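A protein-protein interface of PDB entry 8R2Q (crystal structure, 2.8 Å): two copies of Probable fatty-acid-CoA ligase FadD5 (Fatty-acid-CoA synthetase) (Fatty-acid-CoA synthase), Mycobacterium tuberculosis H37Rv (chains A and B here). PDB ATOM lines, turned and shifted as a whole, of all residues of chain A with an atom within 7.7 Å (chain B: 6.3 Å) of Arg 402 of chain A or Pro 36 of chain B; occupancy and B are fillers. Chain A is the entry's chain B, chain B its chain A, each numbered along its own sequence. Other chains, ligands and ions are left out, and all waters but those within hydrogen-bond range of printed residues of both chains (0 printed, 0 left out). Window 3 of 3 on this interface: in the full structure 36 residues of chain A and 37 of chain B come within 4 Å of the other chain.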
ATOM      1  N   VAL A 375       0.005  19.598   8.303  1.00  0.00           N
ATOM      2  CA  VAL A 375      -1.425  19.761   8.073  1.00  0.00           C
ATOM      3  C   VAL A 375      -2.160  19.670   9.401  1.00  0.00           C
ATOM      4  O   VAL A 375      -2.010  18.691  10.147  1.00  0.00           O
ATOM      5  CB  VAL A 375      -1.933  18.710   7.077  1.00  0.00           C
ATOM      6  CG1 VAL A 375      -3.418  18.893   6.831  1.00  0.00           C
ATOM      7  CG2 VAL A 375      -1.159  18.804   5.775  1.00  0.00           C
ATOM      8  N   THR A 378      -7.637  19.073  11.898  1.00  0.00           N
ATOM      9  CA  THR A 378      -9.020  19.083  11.439  1.00  0.00           C
ATOM     10  C   THR A 378      -9.124  19.149   9.920  1.00  0.00           C
ATOM     11  O   THR A 378     -10.178  19.516   9.392  1.00  0.00           O
ATOM     12  CB  THR A 378      -9.784  20.242  12.075  1.00  0.00           C
ATOM     13  OG1 THR A 378      -9.121  21.477  11.779  1.00  0.00           O
ATOM     14  CG2 THR A 378      -9.860  20.059  13.583  1.00  0.00           C
ATOM     15  N   VAL A 379      -8.053  18.796   9.212  1.00  0.00           N
ATOM     16  CA  VAL A 379      -8.001  18.864   7.756  1.00  0.00           C
ATOM     17  C   VAL A 379      -7.325  17.603   7.237  1.00  0.00           C
ATOM     18  O   VAL A 379      -6.268  17.208   7.740  1.00  0.00           O
ATOM     19  CB  VAL A 379      -7.247  20.117   7.266  1.00  0.00           C
ATOM     20  CG1 VAL A 379      -6.916  19.999   5.787  1.00  0.00           C
ATOM     21  CG2 VAL A 379      -8.066  21.365   7.526  1.00  0.00           C
ATOM     22  N   ALA A 380      -7.934  16.973   6.239  1.00  0.00           N
ATOM     23  CA  ALA A 380      -7.340  15.850   5.527  1.00  0.00           C
ATOM     24  C   ALA A 380      -6.687  16.353   4.248  1.00  0.00           C
ATOM     25  O   ALA A 380      -7.218  17.245   3.582  1.00  0.00           O
ATOM     26  CB  ALA A 380      -8.394  14.794   5.199  1.00  0.00           C
ATOM     27  N   ALA A 381      -5.535  15.781   3.905  1.00  0.00           N
ATOM     28  CA  ALA A 381      -4.768  16.263   2.766  1.00  0.00           C
ATOM     29  C   ALA A 381      -4.104  15.104   2.039  1.00  0.00           C
ATOM     30  O   ALA A 381      -3.699  14.112   2.651  1.00  0.00           O
ATOM     31  CB  ALA A 381      -3.704  17.284   3.195  1.00  0.00           C
ATOM     32  N   ARG A 382      -3.999  15.249   0.718  1.00  0.00           N
ATOM     33  CA  ARG A 382      -3.284  14.314  -0.138  1.00  0.00           C
ATOM     34  C   ARG A 382      -2.422  15.098  -1.117  1.00  0.00           C
ATOM     35  O   ARG A 382      -2.751  16.226  -1.489  1.00  0.00           O
ATOM     36  CB  ARG A 382      -4.234  13.408  -0.929  1.00  0.00           C
ATOM     37  CG  ARG A 382      -5.030  12.422  -0.105  1.00  0.00           C
ATOM     38  CD  ARG A 382      -6.071  11.742  -0.978  1.00  0.00           C
ATOM     39  NE  ARG A 382      -5.481  11.106  -2.149  1.00  0.00           N
ATOM     40  CZ  ARG A 382      -6.160  10.767  -3.235  1.00  0.00           C
ATOM     41  NH1 ARG A 382      -7.454  11.016  -3.348  1.00  0.00           N
ATOM     42  NH2 ARG A 382      -5.522  10.171  -4.239  1.00  0.00           N
ATOM     43  N   VAL A 400      -4.295  18.463  -2.051  1.00  0.00           N
ATOM     44  CA  VAL A 400      -5.745  18.504  -2.149  1.00  0.00           C
ATOM     45  C   VAL A 400      -6.320  18.230  -0.770  1.00  0.00           C
ATOM     46  O   VAL A 400      -5.746  17.473   0.020  1.00  0.00           O
ATOM     47  CB  VAL A 400      -6.279  17.496  -3.192  1.00  0.00           C
ATOM     48  CG1 VAL A 400      -5.767  17.856  -4.576  1.00  0.00           C
ATOM     49  CG2 VAL A 400      -5.872  16.081  -2.830  1.00  0.00           C
ATOM     50  N   TYR A 401      -7.457  18.854  -0.474  1.00  0.00           N
ATOM     51  CA  TYR A 401      -7.985  18.877   0.881  1.00  0.00           C
ATOM     52  C   TYR A 401      -9.400  18.315   0.949  1.00  0.00           C
ATOM     53  O   TYR A 401     -10.174  18.403  -0.008  1.00  0.00           O
ATOM     54  CB  TYR A 401      -8.001  20.300   1.446  1.00  0.00           C
ATOM     55  CG  TYR A 401      -6.650  20.968   1.500  1.00  0.00           C
ATOM     56  CD1 TYR A 401      -5.651  20.494   2.340  1.00  0.00           C
ATOM     57  CD2 TYR A 401      -6.379  22.090   0.726  1.00  0.00           C
ATOM     58  CE1 TYR A 401      -4.414  21.110   2.398  1.00  0.00           C
ATOM     59  CE2 TYR A 401      -5.149  22.713   0.778  1.00  0.00           C
ATOM     60  CZ  TYR A 401      -4.171  22.221   1.615  1.00  0.00           C
ATOM     61  OH  TYR A 401      -2.946  22.845   1.663  1.00  0.00           O
ATOM     62  N   ARG A 402      -9.724  17.744   2.107  1.00  0.00           N
ATOM     63  CA  ARG A 402     -11.095  17.413   2.481  1.00  0.00           C
ATOM     64  C   ARG A 402     -11.290  17.834   3.929  1.00  0.00           C
ATOM     65  O   ARG A 402     -10.550  17.382   4.808  1.00  0.00           O
ATOM     66  CB  ARG A 402     -11.389  15.921   2.305  1.00  0.00           C
ATOM     67  CG  ARG A 402     -12.005  15.570   0.967  1.00  0.00           C
ATOM     68  CD  ARG A 402     -12.964  14.399   1.096  1.00  0.00           C
ATOM     69  NE  ARG A 402     -12.433  13.185   0.490  1.00  0.00           N
ATOM     70  CZ  ARG A 402     -13.060  12.016   0.494  1.00  0.00           C
ATOM     71  NH1 ARG A 402     -14.239  11.867   1.076  1.00  0.00           N
ATOM     72  NH2 ARG A 402     -12.489  10.971  -0.098  1.00  0.00           N
ATOM     73  N   ALA A 403     -12.271  18.700   4.181  1.00  0.00           N
ATOM     74  CA  ALA A 403     -12.481  19.211   5.532  1.00  0.00           C
ATOM     75  C   ALA A 403     -13.854  19.860   5.647  1.00  0.00           C
ATOM     76  O   ALA A 403     -14.408  20.321   4.641  1.00  0.00           O
ATOM     77  CB  ALA A 403     -11.389  20.216   5.907  1.00  0.00           C
ATOM     78  N   PRO A 404     -14.433  19.920   6.852  1.00  0.00           N
ATOM     79  CA  PRO A 404     -15.706  20.642   7.010  1.00  0.00           C
ATOM     80  C   PRO A 404     -15.575  22.142   6.824  1.00  0.00           C
ATOM     81  O   PRO A 404     -16.583  22.807   6.551  1.00  0.00           O
ATOM     82  CB  PRO A 404     -16.137  20.299   8.445  1.00  0.00           C
ATOM     83  CG  PRO A 404     -15.329  19.090   8.818  1.00  0.00           C
ATOM     84  CD  PRO A 404     -14.035  19.227   8.087  1.00  0.00           C
ATOM     85  N   THR A 405     -14.373  22.696   6.963  1.00  0.00           N
ATOM     86  CA  THR A 405     -14.146  24.129   6.857  1.00  0.00           C
ATOM     87  C   THR A 405     -13.850  24.585   5.433  1.00  0.00           C
ATOM     88  O   THR A 405     -13.418  25.726   5.236  1.00  0.00           O
ATOM     89  CB  THR A 405     -13.003  24.548   7.782  1.00  0.00           C
ATOM     90  OG1 THR A 405     -11.924  23.615   7.659  1.00  0.00           O
ATOM     91  CG2 THR A 405     -13.476  24.564   9.213  1.00  0.00           C
ATOM     92  N   LEU A 406     -14.064  23.727   4.440  1.00  0.00           N
ATOM     93  CA  LEU A 406     -13.953  24.150   3.055  1.00  0.00           C
ATOM     94  C   LEU A 406     -15.224  24.874   2.623  1.00  0.00           C
ATOM     95  O   LEU A 406     -16.297  24.706   3.208  1.00  0.00           O
ATOM     96  CB  LEU A 406     -13.689  22.949   2.144  1.00  0.00           C
ATOM     97  CG  LEU A 406     -12.289  22.344   2.237  1.00  0.00           C
ATOM     98  CD1 LEU A 406     -12.241  20.991   1.550  1.00  0.00           C
ATOM     99  CD2 LEU A 406     -11.271  23.290   1.629  1.00  0.00           C
ATOM    100  N   PHE A 421     -13.681  20.795  -6.916  1.00  0.00           N
ATOM    101  CA  PHE A 421     -13.784  19.564  -6.141  1.00  0.00           C
ATOM    102  C   PHE A 421     -13.667  18.323  -7.022  1.00  0.00           C
ATOM    103  O   PHE A 421     -14.303  17.301  -6.752  1.00  0.00           O
ATOM    104  CB  PHE A 421     -15.091  19.535  -5.352  1.00  0.00           C
ATOM    105  CG  PHE A 421     -15.153  20.547  -4.244  1.00  0.00           C
ATOM    106  CD1 PHE A 421     -14.474  20.331  -3.058  1.00  0.00           C
ATOM    107  CD2 PHE A 421     -15.892  21.706  -4.385  1.00  0.00           C
ATOM    108  CE1 PHE A 421     -14.527  21.256  -2.035  1.00  0.00           C
ATOM    109  CE2 PHE A 421     -15.950  22.634  -3.365  1.00  0.00           C
ATOM    110  CZ  PHE A 421     -15.266  22.408  -2.189  1.00  0.00           C
ATOM    111  N   GLY A 423     -12.775  14.923  -8.420  1.00  0.00           N
ATOM    112  CA  GLY A 423     -12.321  13.706  -7.784  1.00  0.00           C
ATOM    113  C   GLY A 423     -12.683  13.566  -6.324  1.00  0.00           C
ATOM    114  O   GLY A 423     -12.239  12.608  -5.684  1.00  0.00           O
ATOM    115  N   GLY A 424     -13.471  14.487  -5.775  1.00  0.00           N
ATOM    116  CA  GLY A 424     -13.858  14.430  -4.381  1.00  0.00           C
ATOM    117  C   GLY A 424     -12.937  15.149  -3.422  1.00  0.00           C
ATOM    118  O   GLY A 424     -13.096  14.991  -2.205  1.00  0.00           O
ATOM    119  N   TRP A 425     -11.979  15.926  -3.923  1.00  0.00           N
ATOM    120  CA  TRP A 425     -11.060  16.680  -3.084  1.00  0.00           C
ATOM    121  C   TRP A 425     -10.918  18.088  -3.646  1.00  0.00           C
ATOM    122  O   TRP A 425     -10.953  18.294  -4.862  1.00  0.00           O
ATOM    123  CB  TRP A 425      -9.681  16.002  -2.998  1.00  0.00           C
ATOM    124  CG  TRP A 425      -9.705  14.665  -2.315  1.00  0.00           C
ATOM    125  CD1 TRP A 425     -10.202  13.497  -2.815  1.00  0.00           C
ATOM    126  CD2 TRP A 425      -9.203  14.357  -1.007  1.00  0.00           C
ATOM    127  NE1 TRP A 425     -10.048  12.486  -1.900  1.00  0.00           N
ATOM    128  CE2 TRP A 425      -9.435  12.987  -0.782  1.00  0.00           C
ATOM    129  CE3 TRP A 425      -8.579  15.109  -0.005  1.00  0.00           C
ATOM    130  CZ2 TRP A 425      -9.073  12.353   0.404  1.00  0.00           C
ATOM    131  CZ3 TRP A 425      -8.217  14.476   1.170  1.00  0.00           C
ATOM    132  CH2 TRP A 425      -8.462  13.111   1.364  1.00  0.00           C
ATOM    133  N   PHE A 426     -10.767  19.058  -2.748  1.00  0.00           N
ATOM    134  CA  PHE A 426     -10.577  20.442  -3.159  1.00  0.00           C
ATOM    135  C   PHE A 426      -9.156  20.638  -3.670  1.00  0.00           C
ATOM    136  O   PHE A 426      -8.195  20.182  -3.045  1.00  0.00           O
ATOM    137  CB  PHE A 426     -10.856  21.396  -2.000  1.00  0.00           C
ATOM    138  CG  PHE A 426     -10.536  22.829  -2.311  1.00  0.00           C
ATOM    139  CD1 PHE A 426     -11.396  23.589  -3.087  1.00  0.00           C
ATOM    140  CD2 PHE A 426      -9.378  23.416  -1.833  1.00  0.00           C
ATOM    141  CE1 PHE A 426     -11.107  24.909  -3.379  1.00  0.00           C
ATOM    142  CE2 PHE A 426      -9.083  24.737  -2.123  1.00  0.00           C
ATOM    143  CZ  PHE A 426      -9.949  25.483  -2.895  1.00  0.00           C
ATOM    144  N   PRO B  36     -10.381  10.485   5.243  1.00  0.00           N
ATOM    145  CA  PRO B  36     -11.252  11.554   4.744  1.00  0.00           C
ATOM    146  C   PRO B  36     -12.183  12.110   5.819  1.00  0.00           C
ATOM    147  O   PRO B  36     -12.489  11.409   6.784  1.00  0.00           O
ATOM    148  CB  PRO B  36     -12.054  10.860   3.641  1.00  0.00           C
ATOM    149  CG  PRO B  36     -11.159   9.773   3.163  1.00  0.00           C
ATOM    150  CD  PRO B  36     -10.419   9.291   4.381  1.00  0.00           C
ATOM    151  N   TYR B  37     -12.621  13.360   5.649  1.00  0.00           N
ATOM    152  CA  TYR B  37     -13.577  13.987   6.553  1.00  0.00           C
ATOM    153  C   TYR B  37     -15.004  13.946   6.012  1.00  0.00           C
ATOM    154  O   TYR B  37     -15.831  14.780   6.400  1.00  0.00           O
ATOM    155  CB  TYR B  37     -13.160  15.428   6.857  1.00  0.00           C
ATOM    156  CG  TYR B  37     -12.567  15.610   8.238  1.00  0.00           C
ATOM    157  CD1 TYR B  37     -13.334  15.392   9.377  1.00  0.00           C
ATOM    158  CD2 TYR B  37     -11.245  16.004   8.405  1.00  0.00           C
ATOM    159  CE1 TYR B  37     -12.801  15.557  10.643  1.00  0.00           C
ATOM    160  CE2 TYR B  37     -10.704  16.172   9.669  1.00  0.00           C
ATOM    161  CZ  TYR B  37     -11.486  15.948  10.784  1.00  0.00           C
ATOM    162  OH  TYR B  37     -10.952  16.114  12.043  1.00  0.00           O
ATOM    163  N   LEU B  38     -15.294  12.999   5.116  1.00  0.00           N
ATOM    164  CA  LEU B  38     -16.640  12.714   4.624  1.00  0.00           C
ATOM    165  C   LEU B  38     -17.401  13.959   4.183  1.00  0.00           C
ATOM    166  O   LEU B  38     -16.831  14.851   3.546  1.00  0.00           O
ATOM    167  CB  LEU B  38     -17.441  11.953   5.686  1.00  0.00           C
ATOM    168  CG  LEU B  38     -17.323  10.423   5.661  1.00  0.00           C
ATOM    169  CD1 LEU B  38     -15.907   9.955   5.979  1.00  0.00           C
ATOM    170  CD2 LEU B  38     -18.329   9.784   6.611  1.00  0.00           C
ATOM    171  N   ALA B  39     -18.688  14.028   4.521  1.00  0.00           N
ATOM    172  CA  ALA B  39     -19.579  15.061   3.994  1.00  0.00           C
ATOM    173  C   ALA B  39     -19.776  16.171   5.028  1.00  0.00           C
ATOM    174  O   ALA B  39     -20.853  16.358   5.599  1.00  0.00           O
ATOM    175  CB  ALA B  39     -20.910  14.443   3.573  1.00  0.00           C
ATOM    176  N   ASN B  46     -14.910  10.270  12.300  1.00  0.00           N
ATOM    177  CA  ASN B  46     -14.256  10.841  11.127  1.00  0.00           C
ATOM    178  C   ASN B  46     -12.864  11.362  11.455  1.00  0.00           C
ATOM    179  O   ASN B  46     -11.971  11.316  10.602  1.00  0.00           O
ATOM    180  CB  ASN B  46     -15.110  11.961  10.534  1.00  0.00           C
ATOM    181  CG  ASN B  46     -16.275  11.435   9.718  1.00  0.00           C
ATOM    182  OD1 ASN B  46     -16.318  10.257   9.362  1.00  0.00           O
ATOM    183  ND2 ASN B  46     -17.221  12.313   9.407  1.00  0.00           N
ATOM    184  N   GLN B  47     -12.662  11.866  12.674  1.00  0.00           N
ATOM    185  CA  GLN B  47     -11.330  12.303  13.076  1.00  0.00           C
ATOM    186  C   GLN B  47     -10.387  11.117  13.216  1.00  0.00           C
ATOM    187  O   GLN B  47      -9.204  11.213  12.868  1.00  0.00           O
ATOM    188  CB  GLN B  47     -11.412  13.090  14.382  1.00  0.00           C
ATOM    189  CG  GLN B  47     -12.343  14.280  14.310  1.00  0.00           C
ATOM    190  CD  GLN B  47     -12.908  14.657  15.661  1.00  0.00           C
ATOM    191  OE1 GLN B  47     -12.467  14.154  16.694  1.00  0.00           O
ATOM    192  NE2 GLN B  47     -13.899  15.539  15.662  1.00  0.00           N
ATOM    193  N   GLU B  49     -10.588   8.337  11.429  1.00  0.00           N
ATOM    194  CA  GLU B  49     -10.240   8.033  10.046  1.00  0.00           C
ATOM    195  C   GLU B  49      -9.219   9.027   9.507  1.00  0.00           C
ATOM    196  O   GLU B  49      -8.276   8.644   8.805  1.00  0.00           O
ATOM    197  CB  GLU B  49     -11.498   8.043   9.175  1.00  0.00           C
ATOM    198  CG  GLU B  49     -12.636   7.161   9.673  1.00  0.00           C
ATOM    199  CD  GLU B  49     -12.548   5.735   9.163  1.00  0.00           C
ATOM    200  OE1 GLU B  49     -11.472   5.343   8.663  1.00  0.00           O
ATOM    201  OE2 GLU B  49     -13.560   5.009   9.253  1.00  0.00           O
ATOM    202  N   ARG B  50      -9.391  10.310   9.833  1.00  0.00           N
ATOM    203  CA  ARG B  50      -8.451  11.334   9.389  1.00  0.00           C
ATOM    204  C   ARG B  50      -7.061  11.090   9.966  1.00  0.00           C
ATOM    205  O   ARG B  50      -6.059  11.176   9.248  1.00  0.00           O
ATOM    206  CB  ARG B  50      -8.979  12.720   9.777  1.00  0.00           C
ATOM    207  CG  ARG B  50      -7.942  13.728  10.288  1.00  0.00           C
ATOM    208  CD  ARG B  50      -7.102  14.297   9.163  1.00  0.00           C
ATOM    209  NE  ARG B  50      -6.178  15.347   9.586  1.00  0.00           N
ATOM    210  CZ  ARG B  50      -5.090  15.154  10.320  1.00  0.00           C
ATOM    211  NH1 ARG B  50      -4.820  13.979  10.864  1.00  0.00           N
ATOM    212  NH2 ARG B  50      -4.247  16.164  10.508  1.00  0.00           N
ATOM    213  N   MET B  53      -5.110   8.208   8.441  1.00  0.00           N
ATOM    214  CA  MET B  53      -4.592   8.476   7.107  1.00  0.00           C
ATOM    215  C   MET B  53      -3.399   9.424   7.125  1.00  0.00           C
ATOM    216  O   MET B  53      -2.421   9.201   6.403  1.00  0.00           O
ATOM    217  CB  MET B  53      -5.697   9.052   6.219  1.00  0.00           C
ATOM    218  CG  MET B  53      -5.199   9.523   4.868  1.00  0.00           C
ATOM    219  SD  MET B  53      -6.418  10.522   4.004  1.00  0.00           S
ATOM    220  CE  MET B  53      -6.911  11.606   5.335  1.00  0.00           C
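Of chain B, only Pro 36 and Tyr 37 come within 4 Å of Arg 402 of chain A. Of the printed residues of chain A, Met 53 of chain B touches Ala 380 (3.5 Å). Of the printed residues of chain B, Thr 378 of chain A touches Tyr 37. Of the printed residues of chain B, Ala 380 of chain A touches Arg 50 and Met 53. Of the printed residues of chain A, Arg 50 of chain B touches Val 375 (3.4 Å), Val 379 (2.6 Å) and Ala 380 (3.96 Å). Glu 49 of chain B touches none of the printed residues of chain A. Val 400 of chain A touches none of the printed residues of chain B. The nearest residue of chain B that does not touch Arg 402 of chain A is Leu 38 of chain B (4.3 Å). The nearest printed residue of chain A that does not touch Pro 36 of chain B is Trp 425 of chain A (4.3 Å). The nearest printed residue of chain A that does not touch Tyr 37 of chain B is Ala 403 of chain A (4.1 Å).
Printed residues of chain A that touch a printed residue of chain B: Val 375, Thr 378, Val 379, Ala 380, Arg 402 and Pro 404. Among the printed residues, 9 pairs touch across the chains. Among the printed residues, no Asp or Glu carboxylate lies within 4 Å of a Lys or Arg side-chain nitrogen of the other chain.
Among the printed residues, pairs that only touch across the chains: Thr 378 of chain A with Tyr 37 of chain B (3.4 Å), Arg 402 of chain A with Pro 36 of chain B (3.5 Å), Ala 380 of chain A with Met 53 of chain B (3.5 Å), Val 379 of chain A with Tyr 37 of chain B (3.8 Å), Arg 402 of chain A with Tyr 37 of chain B (3.9 Å), Pro 404 of chain A with Tyr 37 of chain B (3.9 Å) and Ala 380 of chain A with Arg 50 of chain B (3.96 Å).
The backbone carbonyl oxygen (O) of Val 379 of chain A is in hydrogen-bond range of the guanidinium group (NE) of Arg 50 of chain B (2.6 Å). NH2 of Arg 50 of chain B sits at hydrogen-bond distance from O of Val 375 of chain A (3.4 Å).
No position is printed for both chains. Of the 9 pairs that touch across the chains among the printed residues, none has its exchanged pair printed and touching as well.
The backbone carbonyl oxygen of Gly 424 of chain A is in hydrogen-bond range of the guanidinium group of Arg 402 of chain A (3.3 Å). O of Ala 380 of chain A lies within hydrogen-bond range of N of Arg 402 of chain A, 3.0 Å away.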
